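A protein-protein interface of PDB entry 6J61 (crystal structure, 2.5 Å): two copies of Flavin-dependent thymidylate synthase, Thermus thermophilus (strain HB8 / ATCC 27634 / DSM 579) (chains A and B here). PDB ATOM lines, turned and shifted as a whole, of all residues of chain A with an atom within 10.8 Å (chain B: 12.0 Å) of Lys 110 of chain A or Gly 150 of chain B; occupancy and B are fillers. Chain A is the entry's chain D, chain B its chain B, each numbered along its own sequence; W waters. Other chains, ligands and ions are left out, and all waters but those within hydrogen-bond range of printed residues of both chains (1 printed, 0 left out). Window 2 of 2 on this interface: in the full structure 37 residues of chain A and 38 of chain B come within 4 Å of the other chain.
N of Ala 152 of chain B is in hydrogen-bond range of O of Arg 109 of chain A, at 2.7 Å.
The guanidinium group (NH1) of Arg 109 of chain A is in salt-bridge range of the side-chain carboxylate (OE2) of Glu 154 of chain B.
The guanidinium group (NH1) of Arg 109 of chain A lies within hydrogen-bond range of the side-chain sulfur (SD) of Met 155 of chain B.
The backbone carbonyl oxygen (O) of Gly 150 of chain B lies within hydrogen-bond range of the backbone NH (N) of Gln 111 of chain A (3.3 Å).
The backbone NH (N) of Ala 152 of chain B sits close to the backbone NH (N) of Gln 111 of chain A (3.5 Å).
O of Glu 154 of chain B lies within hydrogen-bond range of NE of Arg 157 of chain B (2.7 Å).
The side-chain carboxylate of Glu 192 of chain A lies within salt-bridge range of the guanidinium group of Arg 109 of chain A (2.5 Å).
O of Leu 146 of chain B is in hydrogen-bond range of N of Val 151 of chain B (2.9 Å).
The side-chain carboxylate of Glu 154 of chain B is in salt-bridge range of the guanidinium group of Arg 94 of chain B (2.6 Å).
Among the printed residues, merely in contact across the chains: Arg 109 of chain A with Val 151 of chain B, Phe 108 of chain A with Val 151 of chain B, Pro 105 of chain A with Met 155 of chain B, Phe 108 of chain A with Met 155 of chain B, Lys 110 of chain A with Gly 150 of chain B, Ala 107 of chain A with Met 155 of chain B, Leu 131 of chain A with Ala 145 of chain B, Leu 131 of chain A with Ala 142 of chain B, Phe 108 of chain A with Leu 146 of chain B and Lys 110 of chain A with Ala 152 of chain B.
Of the printed residues of chain B, Phe 108 of chain A touches Leu 146, Val 151 and Met 155.
Of the printed residues of chain B, Arg 109 of chain A touches Val 151 (3.3 Å), Ala 152 (2.7 Å), Glu 154 (3.2 Å) and Met 155 (2.9 Å).
Gln 111 of chain A touches just these residues of chain B: Gly 150 (3.3 Å) and Ala 152 (3.4 Å).
Of the printed residues of chain A, Ala 145 of chain B touches Leu 131 (3.6 Å).
Of chain A, only Lys 110 (3.6 Å) and Gln 111 (3.3 Å) come within 4 Å of Gly 150 of chain B.
Val 151 of chain B touches just these residues of chain A: Phe 108 (3.3 Å) and Arg 109 (3.3 Å).
Of the printed residues of chain A, Ala 152 of chain B touches Arg 109 (2.7 Å), Lys 110 (3.996 Å) and Gln 111 (3.4 Å).
The nearest printed residue of chain B that does not touch Lys 110 of chain A is Val 151 of chain B (4.5 Å).
Hydrophobic or aromatic side chains of chain A within 4 Å of the printed part of chain B: Pro 105, Phe 108 and Leu 131.
Of the 20 printed residues of chain B, 8 touch a printed residue of chain A.
Hydrophobic or aromatic side chains of chain B that line the printed part of chain A: Ala 142, Ala 145, Leu 146, Val 151, Ala 152 and Met 155.
Among the printed residues, 15 pairs touch across the chains.
No position is printed for both chains.
Of the 15 pairs that touch across the chains among the printed residues, none has its exchanged pair printed and touching as well.
Water W1 lies within hydrogen-bond range of N of Trp 191 of chain A (3.2 Å) and OE2 of Glu 154 of chain B (3.3 Å).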
ATOM      1  N   PRO A 105      19.210  -6.584 -26.566  1.00  0.00           N
ATOM      2  CA  PRO A 105      19.504  -5.264 -26.007  1.00  0.00           C
ATOM      3  C   PRO A 105      20.617  -5.186 -24.978  1.00  0.00           C
ATOM      4  O   PRO A 105      20.788  -6.084 -24.147  1.00  0.00           O
ATOM      5  CB  PRO A 105      18.162  -4.820 -25.434  1.00  0.00           C
ATOM      6  CG  PRO A 105      17.485  -6.109 -25.122  1.00  0.00           C
ATOM      7  CD  PRO A 105      17.804  -6.938 -26.332  1.00  0.00           C
ATOM      8  N   GLU A 106      21.381  -4.099 -25.068  1.00  0.00           N
ATOM      9  CA  GLU A 106      22.462  -3.825 -24.132  1.00  0.00           C
ATOM     10  C   GLU A 106      21.776  -3.853 -22.771  1.00  0.00           C
ATOM     11  O   GLU A 106      22.209  -4.532 -21.839  1.00  0.00           O
ATOM     12  CB  GLU A 106      23.026  -2.426 -24.396  1.00  0.00           C
ATOM     13  CG  GLU A 106      23.892  -1.865 -23.274  1.00  0.00           C
ATOM     14  CD  GLU A 106      25.274  -2.485 -23.223  1.00  0.00           C
ATOM     15  OE1 GLU A 106      25.375  -3.726 -23.062  1.00  0.00           O
ATOM     16  OE2 GLU A 106      26.261  -1.721 -23.343  1.00  0.00           O
ATOM     17  N   ALA A 107      20.679  -3.107 -22.688  1.00  0.00           N
ATOM     18  CA  ALA A 107      19.879  -3.018 -21.477  1.00  0.00           C
ATOM     19  C   ALA A 107      18.467  -2.626 -21.884  1.00  0.00           C
ATOM     20  O   ALA A 107      18.262  -2.053 -22.957  1.00  0.00           O
ATOM     21  CB  ALA A 107      20.460  -1.973 -20.544  1.00  0.00           C
ATOM     22  N   PHE A 108      17.496  -2.942 -21.034  1.00  0.00           N
ATOM     23  CA  PHE A 108      16.110  -2.599 -21.314  1.00  0.00           C
ATOM     24  C   PHE A 108      15.763  -1.201 -20.822  1.00  0.00           C
ATOM     25  O   PHE A 108      16.084  -0.833 -19.695  1.00  0.00           O
ATOM     26  CB  PHE A 108      15.179  -3.615 -20.666  1.00  0.00           C
ATOM     27  CG  PHE A 108      14.942  -4.829 -21.503  1.00  0.00           C
ATOM     28  CD1 PHE A 108      14.136  -4.758 -22.631  1.00  0.00           C
ATOM     29  CD2 PHE A 108      15.524  -6.043 -21.169  1.00  0.00           C
ATOM     30  CE1 PHE A 108      13.910  -5.883 -23.419  1.00  0.00           C
ATOM     31  CE2 PHE A 108      15.309  -7.174 -21.944  1.00  0.00           C
ATOM     32  CZ  PHE A 108      14.498  -7.096 -23.075  1.00  0.00           C
ATOM     33  N   ARG A 109      15.115  -0.418 -21.678  1.00  0.00           N
ATOM     34  CA  ARG A 109      14.715   0.934 -21.315  1.00  0.00           C
ATOM     35  C   ARG A 109      13.366   0.896 -20.601  1.00  0.00           C
ATOM     36  O   ARG A 109      12.505   0.074 -20.921  1.00  0.00           O
ATOM     37  CB  ARG A 109      14.652   1.817 -22.565  1.00  0.00           C
ATOM     38  CG  ARG A 109      16.010   2.390 -22.964  1.00  0.00           C
ATOM     39  CD  ARG A 109      15.990   3.163 -24.288  1.00  0.00           C
ATOM     40  NE  ARG A 109      16.319   2.309 -25.428  1.00  0.00           N
ATOM     41  CZ  ARG A 109      15.467   1.484 -26.024  1.00  0.00           C
ATOM     42  NH1 ARG A 109      14.217   1.400 -25.599  1.00  0.00           N
ATOM     43  NH2 ARG A 109      15.868   0.734 -27.037  1.00  0.00           N
ATOM     44  N   LYS A 110      13.192   1.781 -19.624  1.00  0.00           N
ATOM     45  CA  LYS A 110      11.956   1.837 -18.845  1.00  0.00           C
ATOM     46  C   LYS A 110      11.032   2.968 -19.293  1.00  0.00           C
ATOM     47  O   LYS A 110      11.426   4.133 -19.303  1.00  0.00           O
ATOM     48  CB  LYS A 110      12.286   2.025 -17.359  1.00  0.00           C
ATOM     49  CG  LYS A 110      13.279   1.021 -16.787  1.00  0.00           C
ATOM     50  CD  LYS A 110      13.755   1.458 -15.406  1.00  0.00           C
ATOM     51  CE  LYS A 110      14.908   0.597 -14.903  1.00  0.00           C
ATOM     52  NZ  LYS A 110      15.431   1.066 -13.583  1.00  0.00           N
ATOM     53  N   GLN A 111       9.799   2.621 -19.648  1.00  0.00           N
ATOM     54  CA  GLN A 111       8.811   3.609 -20.078  1.00  0.00           C
ATOM     55  C   GLN A 111       7.412   3.003 -20.088  1.00  0.00           C
ATOM     56  O   GLN A 111       6.749   2.955 -21.125  1.00  0.00           O
ATOM     57  CB  GLN A 111       9.151   4.138 -21.478  1.00  0.00           C
ATOM     58  CG  GLN A 111      10.182   5.262 -21.515  1.00  0.00           C
ATOM     59  CD  GLN A 111      10.714   5.530 -22.920  1.00  0.00           C
ATOM     60  OE1 GLN A 111      11.380   4.681 -23.516  1.00  0.00           O
ATOM     61  NE2 GLN A 111      10.417   6.712 -23.451  1.00  0.00           N
ATOM     62  N   LEU A 131      14.254 -14.417 -20.840  1.00  0.00           N
ATOM     63  CA  LEU A 131      12.876 -14.389 -21.332  1.00  0.00           C
ATOM     64  C   LEU A 131      12.868 -14.034 -22.819  1.00  0.00           C
ATOM     65  O   LEU A 131      12.089 -14.589 -23.603  1.00  0.00           O
ATOM     66  CB  LEU A 131      12.043 -13.375 -20.531  1.00  0.00           C
ATOM     67  CG  LEU A 131      10.535 -13.244 -20.827  1.00  0.00           C
ATOM     68  CD1 LEU A 131       9.844 -14.605 -20.761  1.00  0.00           C
ATOM     69  CD2 LEU A 131       9.911 -12.280 -19.824  1.00  0.00           C
ATOM     70  N   TRP A 191      15.937   4.891 -29.857  1.00  0.00           N
ATOM     71  CA  TRP A 191      17.356   4.685 -29.598  1.00  0.00           C
ATOM     72  C   TRP A 191      18.050   3.781 -30.612  1.00  0.00           C
ATOM     73  O   TRP A 191      19.093   4.152 -31.154  1.00  0.00           O
ATOM     74  CB  TRP A 191      17.546   4.100 -28.192  1.00  0.00           C
ATOM     75  CG  TRP A 191      18.983   3.968 -27.776  1.00  0.00           C
ATOM     76  CD1 TRP A 191      19.769   4.939 -27.228  1.00  0.00           C
ATOM     77  CD2 TRP A 191      19.830   2.819 -27.958  1.00  0.00           C
ATOM     78  NE1 TRP A 191      21.056   4.472 -27.064  1.00  0.00           N
ATOM     79  CE2 TRP A 191      21.121   3.176 -27.505  1.00  0.00           C
ATOM     80  CE3 TRP A 191      19.622   1.527 -28.467  1.00  0.00           C
ATOM     81  CZ2 TRP A 191      22.204   2.290 -27.544  1.00  0.00           C
ATOM     82  CZ3 TRP A 191      20.703   0.640 -28.509  1.00  0.00           C
ATOM     83  CH2 TRP A 191      21.978   1.030 -28.048  1.00  0.00           C
ATOM     84  N   GLU A 192      17.490   2.596 -30.859  1.00  0.00           N
ATOM     85  CA  GLU A 192      18.093   1.654 -31.807  1.00  0.00           C
ATOM     86  C   GLU A 192      18.431   2.303 -33.145  1.00  0.00           C
ATOM     87  O   GLU A 192      19.566   2.208 -33.610  1.00  0.00           O
ATOM     88  CB  GLU A 192      17.170   0.455 -32.080  1.00  0.00           C
ATOM     89  CG  GLU A 192      17.224  -0.687 -31.072  1.00  0.00           C
ATOM     90  CD  GLU A 192      16.771  -0.276 -29.684  1.00  0.00           C
ATOM     91  OE1 GLU A 192      15.816   0.520 -29.573  1.00  0.00           O
ATOM     92  OE2 GLU A 192      17.369  -0.762 -28.706  1.00  0.00           O
ATOM     93  N   ARG B  94       5.244   1.872 -31.069  1.00  0.00           N
ATOM     94  CA  ARG B  94       5.917   2.699 -30.073  1.00  0.00           C
ATOM     95  C   ARG B  94       4.922   3.357 -29.117  1.00  0.00           C
ATOM     96  O   ARG B  94       4.992   3.175 -27.898  1.00  0.00           O
ATOM     97  CB  ARG B  94       6.757   3.794 -30.751  1.00  0.00           C
ATOM     98  CG  ARG B  94       7.908   3.300 -31.633  1.00  0.00           C
ATOM     99  CD  ARG B  94       8.851   4.451 -31.997  1.00  0.00           C
ATOM    100  NE  ARG B  94       9.716   4.807 -30.880  1.00  0.00           N
ATOM    101  CZ  ARG B  94      10.326   5.981 -30.728  1.00  0.00           C
ATOM    102  NH1 ARG B  94      10.174   6.950 -31.620  1.00  0.00           N
ATOM    103  NH2 ARG B  94      11.105   6.184 -29.677  1.00  0.00           N
ATOM    104  N   ILE B  97      -0.376   0.075 -27.545  1.00  0.00           N
ATOM    105  CA  ILE B  97      -0.229  -1.333 -27.200  1.00  0.00           C
ATOM    106  C   ILE B  97      -0.902  -2.163 -28.293  1.00  0.00           C
ATOM    107  O   ILE B  97      -1.969  -1.807 -28.800  1.00  0.00           O
ATOM    108  CB  ILE B  97      -0.875  -1.657 -25.839  1.00  0.00           C
ATOM    109  CG1 ILE B  97      -0.479  -3.071 -25.415  1.00  0.00           C
ATOM    110  CG2 ILE B  97      -2.389  -1.541 -25.933  1.00  0.00           C
ATOM    111  CD1 ILE B  97      -0.815  -3.403 -23.977  1.00  0.00           C
ATOM    112  N   GLY B 141       3.117 -13.698 -24.312  1.00  0.00           N
ATOM    113  CA  GLY B 141       3.278 -13.836 -22.878  1.00  0.00           C
ATOM    114  C   GLY B 141       4.417 -12.971 -22.383  1.00  0.00           C
ATOM    115  O   GLY B 141       4.269 -12.216 -21.419  1.00  0.00           O
ATOM    116  N   ALA B 142       5.558 -13.080 -23.054  1.00  0.00           N
ATOM    117  CA  ALA B 142       6.733 -12.306 -22.693  1.00  0.00           C
ATOM    118  C   ALA B 142       6.425 -10.834 -22.901  1.00  0.00           C
ATOM    119  O   ALA B 142       7.026  -9.966 -22.266  1.00  0.00           O
ATOM    120  CB  ALA B 142       7.919 -12.722 -23.551  1.00  0.00           C
ATOM    121  N   TYR B 143       5.477 -10.560 -23.792  1.00  0.00           N
ATOM    122  CA  TYR B 143       5.083  -9.189 -24.085  1.00  0.00           C
ATOM    123  C   TYR B 143       4.534  -8.540 -22.819  1.00  0.00           C
ATOM    124  O   TYR B 143       5.092  -7.554 -22.318  1.00  0.00           O
ATOM    125  CB  TYR B 143       4.026  -9.180 -25.198  1.00  0.00           C
ATOM    126  CG  TYR B 143       3.635  -7.806 -25.700  1.00  0.00           C
ATOM    127  CD1 TYR B 143       4.602  -6.827 -25.939  1.00  0.00           C
ATOM    128  CD2 TYR B 143       2.301  -7.494 -25.968  1.00  0.00           C
ATOM    129  CE1 TYR B 143       4.250  -5.570 -26.434  1.00  0.00           C
ATOM    130  CE2 TYR B 143       1.937  -6.244 -26.463  1.00  0.00           C
ATOM    131  CZ  TYR B 143       2.918  -5.288 -26.694  1.00  0.00           C
ATOM    132  OH  TYR B 143       2.573  -4.052 -27.187  1.00  0.00           O
ATOM    133  N   ARG B 144       3.447  -9.107 -22.296  1.00  0.00           N
ATOM    134  CA  ARG B 144       2.834  -8.582 -21.085  1.00  0.00           C
ATOM    135  C   ARG B 144       3.853  -8.608 -19.955  1.00  0.00           C
ATOM    136  O   ARG B 144       3.906  -7.693 -19.131  1.00  0.00           O
ATOM    137  CB  ARG B 144       1.596  -9.400 -20.707  1.00  0.00           C
ATOM    138  CG  ARG B 144       0.493  -9.359 -21.759  1.00  0.00           C
ATOM    139  CD  ARG B 144      -0.863  -9.761 -21.184  1.00  0.00           C
ATOM    140  NE  ARG B 144      -1.418  -8.751 -20.278  1.00  0.00           N
ATOM    141  CZ  ARG B 144      -1.788  -7.523 -20.646  1.00  0.00           C
ATOM    142  NH1 ARG B 144      -1.668  -7.130 -21.912  1.00  0.00           N
ATOM    143  NH2 ARG B 144      -2.282  -6.683 -19.746  1.00  0.00           N
ATOM    144  N   ALA B 145       4.670  -9.654 -19.928  1.00  0.00           N
ATOM    145  CA  ALA B 145       5.703  -9.788 -18.907  1.00  0.00           C
ATOM    146  C   ALA B 145       6.587  -8.543 -18.890  1.00  0.00           C
ATOM    147  O   ALA B 145       6.705  -7.863 -17.867  1.00  0.00           O
ATOM    148  CB  ALA B 145       6.544 -11.026 -19.184  1.00  0.00           C
ATOM    149  N   LEU B 146       7.205  -8.255 -20.034  1.00  0.00           N
ATOM    150  CA  LEU B 146       8.078  -7.094 -20.183  1.00  0.00           C
ATOM    151  C   LEU B 146       7.302  -5.831 -19.836  1.00  0.00           C
ATOM    152  O   LEU B 146       7.802  -4.963 -19.119  1.00  0.00           O
ATOM    153  CB  LEU B 146       8.605  -7.013 -21.622  1.00  0.00           C
ATOM    154  CG  LEU B 146       9.581  -8.124 -22.028  1.00  0.00           C
ATOM    155  CD1 LEU B 146       9.486  -8.375 -23.510  1.00  0.00           C
ATOM    156  CD2 LEU B 146      11.001  -7.756 -21.626  1.00  0.00           C
ATOM    157  N   LEU B 147       6.080  -5.731 -20.350  1.00  0.00           N
ATOM    158  CA  LEU B 147       5.240  -4.576 -20.070  1.00  0.00           C
ATOM    159  C   LEU B 147       5.009  -4.471 -18.562  1.00  0.00           C
ATOM    160  O   LEU B 147       5.217  -3.411 -17.968  1.00  0.00           O
ATOM    161  CB  LEU B 147       3.904  -4.703 -20.805  1.00  0.00           C
ATOM    162  CG  LEU B 147       4.000  -4.521 -22.320  1.00  0.00           C
ATOM    163  CD1 LEU B 147       2.672  -4.843 -22.979  1.00  0.00           C
ATOM    164  CD2 LEU B 147       4.431  -3.087 -22.620  1.00  0.00           C
ATOM    165  N   GLU B 148       4.588  -5.581 -17.957  1.00  0.00           N
ATOM    166  CA  GLU B 148       4.336  -5.650 -16.520  1.00  0.00           C
ATOM    167  C   GLU B 148       5.541  -5.155 -15.718  1.00  0.00           C
ATOM    168  O   GLU B 148       5.397  -4.393 -14.760  1.00  0.00           O
ATOM    169  CB  GLU B 148       4.019  -7.091 -16.108  1.00  0.00           C
ATOM    170  CG  GLU B 148       2.615  -7.297 -15.561  1.00  0.00           C
ATOM    171  CD  GLU B 148       1.562  -7.424 -16.651  1.00  0.00           C
ATOM    172  OE1 GLU B 148       1.564  -8.453 -17.364  1.00  0.00           O
ATOM    173  OE2 GLU B 148       0.733  -6.499 -16.794  1.00  0.00           O
ATOM    174  N   LYS B 149       6.731  -5.599 -16.110  1.00  0.00           N
ATOM    175  CA  LYS B 149       7.948  -5.187 -15.428  1.00  0.00           C
ATOM    176  C   LYS B 149       8.249  -3.726 -15.733  1.00  0.00           C
ATOM    177  O   LYS B 149       9.206  -3.161 -15.211  1.00  0.00           O
ATOM    178  CB  LYS B 149       9.131  -6.061 -15.854  1.00  0.00           C
ATOM    179  CG  LYS B 149       8.939  -7.552 -15.601  1.00  0.00           C
ATOM    180  CD  LYS B 149      10.278  -8.284 -15.581  1.00  0.00           C
ATOM    181  CE  LYS B 149      11.163  -7.789 -14.431  1.00  0.00           C
ATOM    182  NZ  LYS B 149      12.474  -8.491 -14.328  1.00  0.00           N
ATOM    183  N   GLY B 150       7.432  -3.123 -16.594  1.00  0.00           N
ATOM    184  CA  GLY B 150       7.605  -1.721 -16.939  1.00  0.00           C
ATOM    185  C   GLY B 150       8.616  -1.354 -18.015  1.00  0.00           C
ATOM    186  O   GLY B 150       9.083  -0.215 -18.055  1.00  0.00           O
ATOM    187  N   VAL B 151       8.961  -2.293 -18.891  1.00  0.00           N
ATOM    188  CA  VAL B 151       9.920  -2.001 -19.952  1.00  0.00           C
ATOM    189  C   VAL B 151       9.237  -1.201 -21.057  1.00  0.00           C
ATOM    190  O   VAL B 151       8.078  -1.459 -21.387  1.00  0.00           O
ATOM    191  CB  VAL B 151      10.494  -3.290 -20.565  1.00  0.00           C
ATOM    192  CG1 VAL B 151      11.509  -2.942 -21.634  1.00  0.00           C
ATOM    193  CG2 VAL B 151      11.135  -4.139 -19.484  1.00  0.00           C
ATOM    194  N   ALA B 152       9.955  -0.230 -21.618  1.00  0.00           N
ATOM    195  CA  ALA B 152       9.432   0.622 -22.690  1.00  0.00           C
ATOM    196  C   ALA B 152       8.685  -0.165 -23.770  1.00  0.00           C
ATOM    197  O   ALA B 152       9.200  -1.147 -24.303  1.00  0.00           O
ATOM    198  CB  ALA B 152      10.575   1.403 -23.321  1.00  0.00           C
ATOM    199  N   ARG B 153       7.475   0.279 -24.096  1.00  0.00           N
ATOM    200  CA  ARG B 153       6.665  -0.393 -25.103  1.00  0.00           C
ATOM    201  C   ARG B 153       7.410  -0.622 -26.417  1.00  0.00           C
ATOM    202  O   ARG B 153       7.252  -1.669 -27.053  1.00  0.00           O
ATOM    203  CB  ARG B 153       5.390   0.405 -25.378  1.00  0.00           C
ATOM    204  CG  ARG B 153       4.120  -0.273 -24.894  1.00  0.00           C
ATOM    205  CD  ARG B 153       2.876   0.426 -25.424  1.00  0.00           C
ATOM    206  NE  ARG B 153       2.794   1.822 -24.997  1.00  0.00           N
ATOM    207  CZ  ARG B 153       2.611   2.226 -23.741  1.00  0.00           C
ATOM    208  NH1 ARG B 153       2.485   1.343 -22.759  1.00  0.00           N
ATOM    209  NH2 ARG B 153       2.554   3.522 -23.465  1.00  0.00           N
ATOM    210  N   GLU B 154       8.221   0.349 -26.823  1.00  0.00           N
ATOM    211  CA  GLU B 154       8.973   0.225 -28.067  1.00  0.00           C
ATOM    212  C   GLU B 154       9.928  -0.973 -28.110  1.00  0.00           C
ATOM    213  O   GLU B 154      10.306  -1.421 -29.187  1.00  0.00           O
ATOM    214  CB  GLU B 154       9.741   1.520 -28.353  1.00  0.00           C
ATOM    215  CG  GLU B 154      10.706   1.958 -27.263  1.00  0.00           C
ATOM    216  CD  GLU B 154      11.368   3.287 -27.590  1.00  0.00           C
ATOM    217  OE1 GLU B 154      10.648   4.205 -28.031  1.00  0.00           O
ATOM    218  OE2 GLU B 154      12.597   3.424 -27.403  1.00  0.00           O
ATOM    219  N   MET B 155      10.324  -1.490 -26.950  1.00  0.00           N
ATOM    220  CA  MET B 155      11.215  -2.653 -26.896  1.00  0.00           C
ATOM    221  C   MET B 155      10.434  -3.923 -26.572  1.00  0.00           C
ATOM    222  O   MET B 155      10.911  -5.024 -26.797  1.00  0.00           O
ATOM    223  CB  MET B 155      12.284  -2.471 -25.828  1.00  0.00           C
ATOM    224  CG  MET B 155      13.283  -1.380 -26.090  1.00  0.00           C
ATOM    225  SD  MET B 155      14.527  -1.336 -24.773  1.00  0.00           S
ATOM    226  CE  MET B 155      15.460  -2.815 -25.152  1.00  0.00           C
ATOM    227  N   ALA B 156       9.235  -3.768 -26.030  1.00  0.00           N
ATOM    228  CA  ALA B 156       8.423  -4.916 -25.675  1.00  0.00           C
ATOM    229  C   ALA B 156       7.893  -5.665 -26.897  1.00  0.00           C
ATOM    230  O   ALA B 156       8.045  -6.886 -26.996  1.00  0.00           O
ATOM    231  CB  ALA B 156       7.269  -4.474 -24.791  1.00  0.00           C
ATOM    232  N   ARG B 157       7.265  -4.938 -27.821  1.00  0.00           N
ATOM    233  CA  ARG B 157       6.709  -5.548 -29.032  1.00  0.00           C
ATOM    234  C   ARG B 157       7.795  -6.245 -29.834  1.00  0.00           C
ATOM    235  O   ARG B 157       7.530  -6.987 -30.777  1.00  0.00           O
ATOM    236  CB  ARG B 157       6.008  -4.487 -29.891  1.00  0.00           C
ATOM    237  CG  ARG B 157       6.804  -3.195 -30.124  1.00  0.00           C
ATOM    238  CD  ARG B 157       8.065  -3.421 -30.951  1.00  0.00           C
ATOM    239  NE  ARG B 157       8.733  -2.161 -31.266  1.00  0.00           N
ATOM    240  CZ  ARG B 157       8.298  -1.278 -32.161  1.00  0.00           C
ATOM    241  NH1 ARG B 157       7.186  -1.509 -32.854  1.00  0.00           N
ATOM    242  NH2 ARG B 157       8.967  -0.148 -32.345  1.00  0.00           N
ATOM    243  N   MET B 158       9.029  -5.992 -29.438  1.00  0.00           N
ATOM    244  CA  MET B 158      10.187  -6.575 -30.083  1.00  0.00           C
ATOM    245  C   MET B 158      10.055  -8.104 -30.211  1.00  0.00           C
ATOM    246  O   MET B 158      10.381  -8.679 -31.254  1.00  0.00           O
ATOM    247  CB  MET B 158      11.423  -6.206 -29.264  1.00  0.00           C
ATOM    248  CG  MET B 158      12.746  -6.544 -29.882  1.00  0.00           C
ATOM    249  SD  MET B 158      14.087  -6.176 -28.744  1.00  0.00           S
ATOM    250  CE  MET B 158      13.951  -4.357 -28.610  1.00  0.00           C
HETATM  251  O   HOH W   1      14.565   6.042 -27.150  1.00  0.00           O
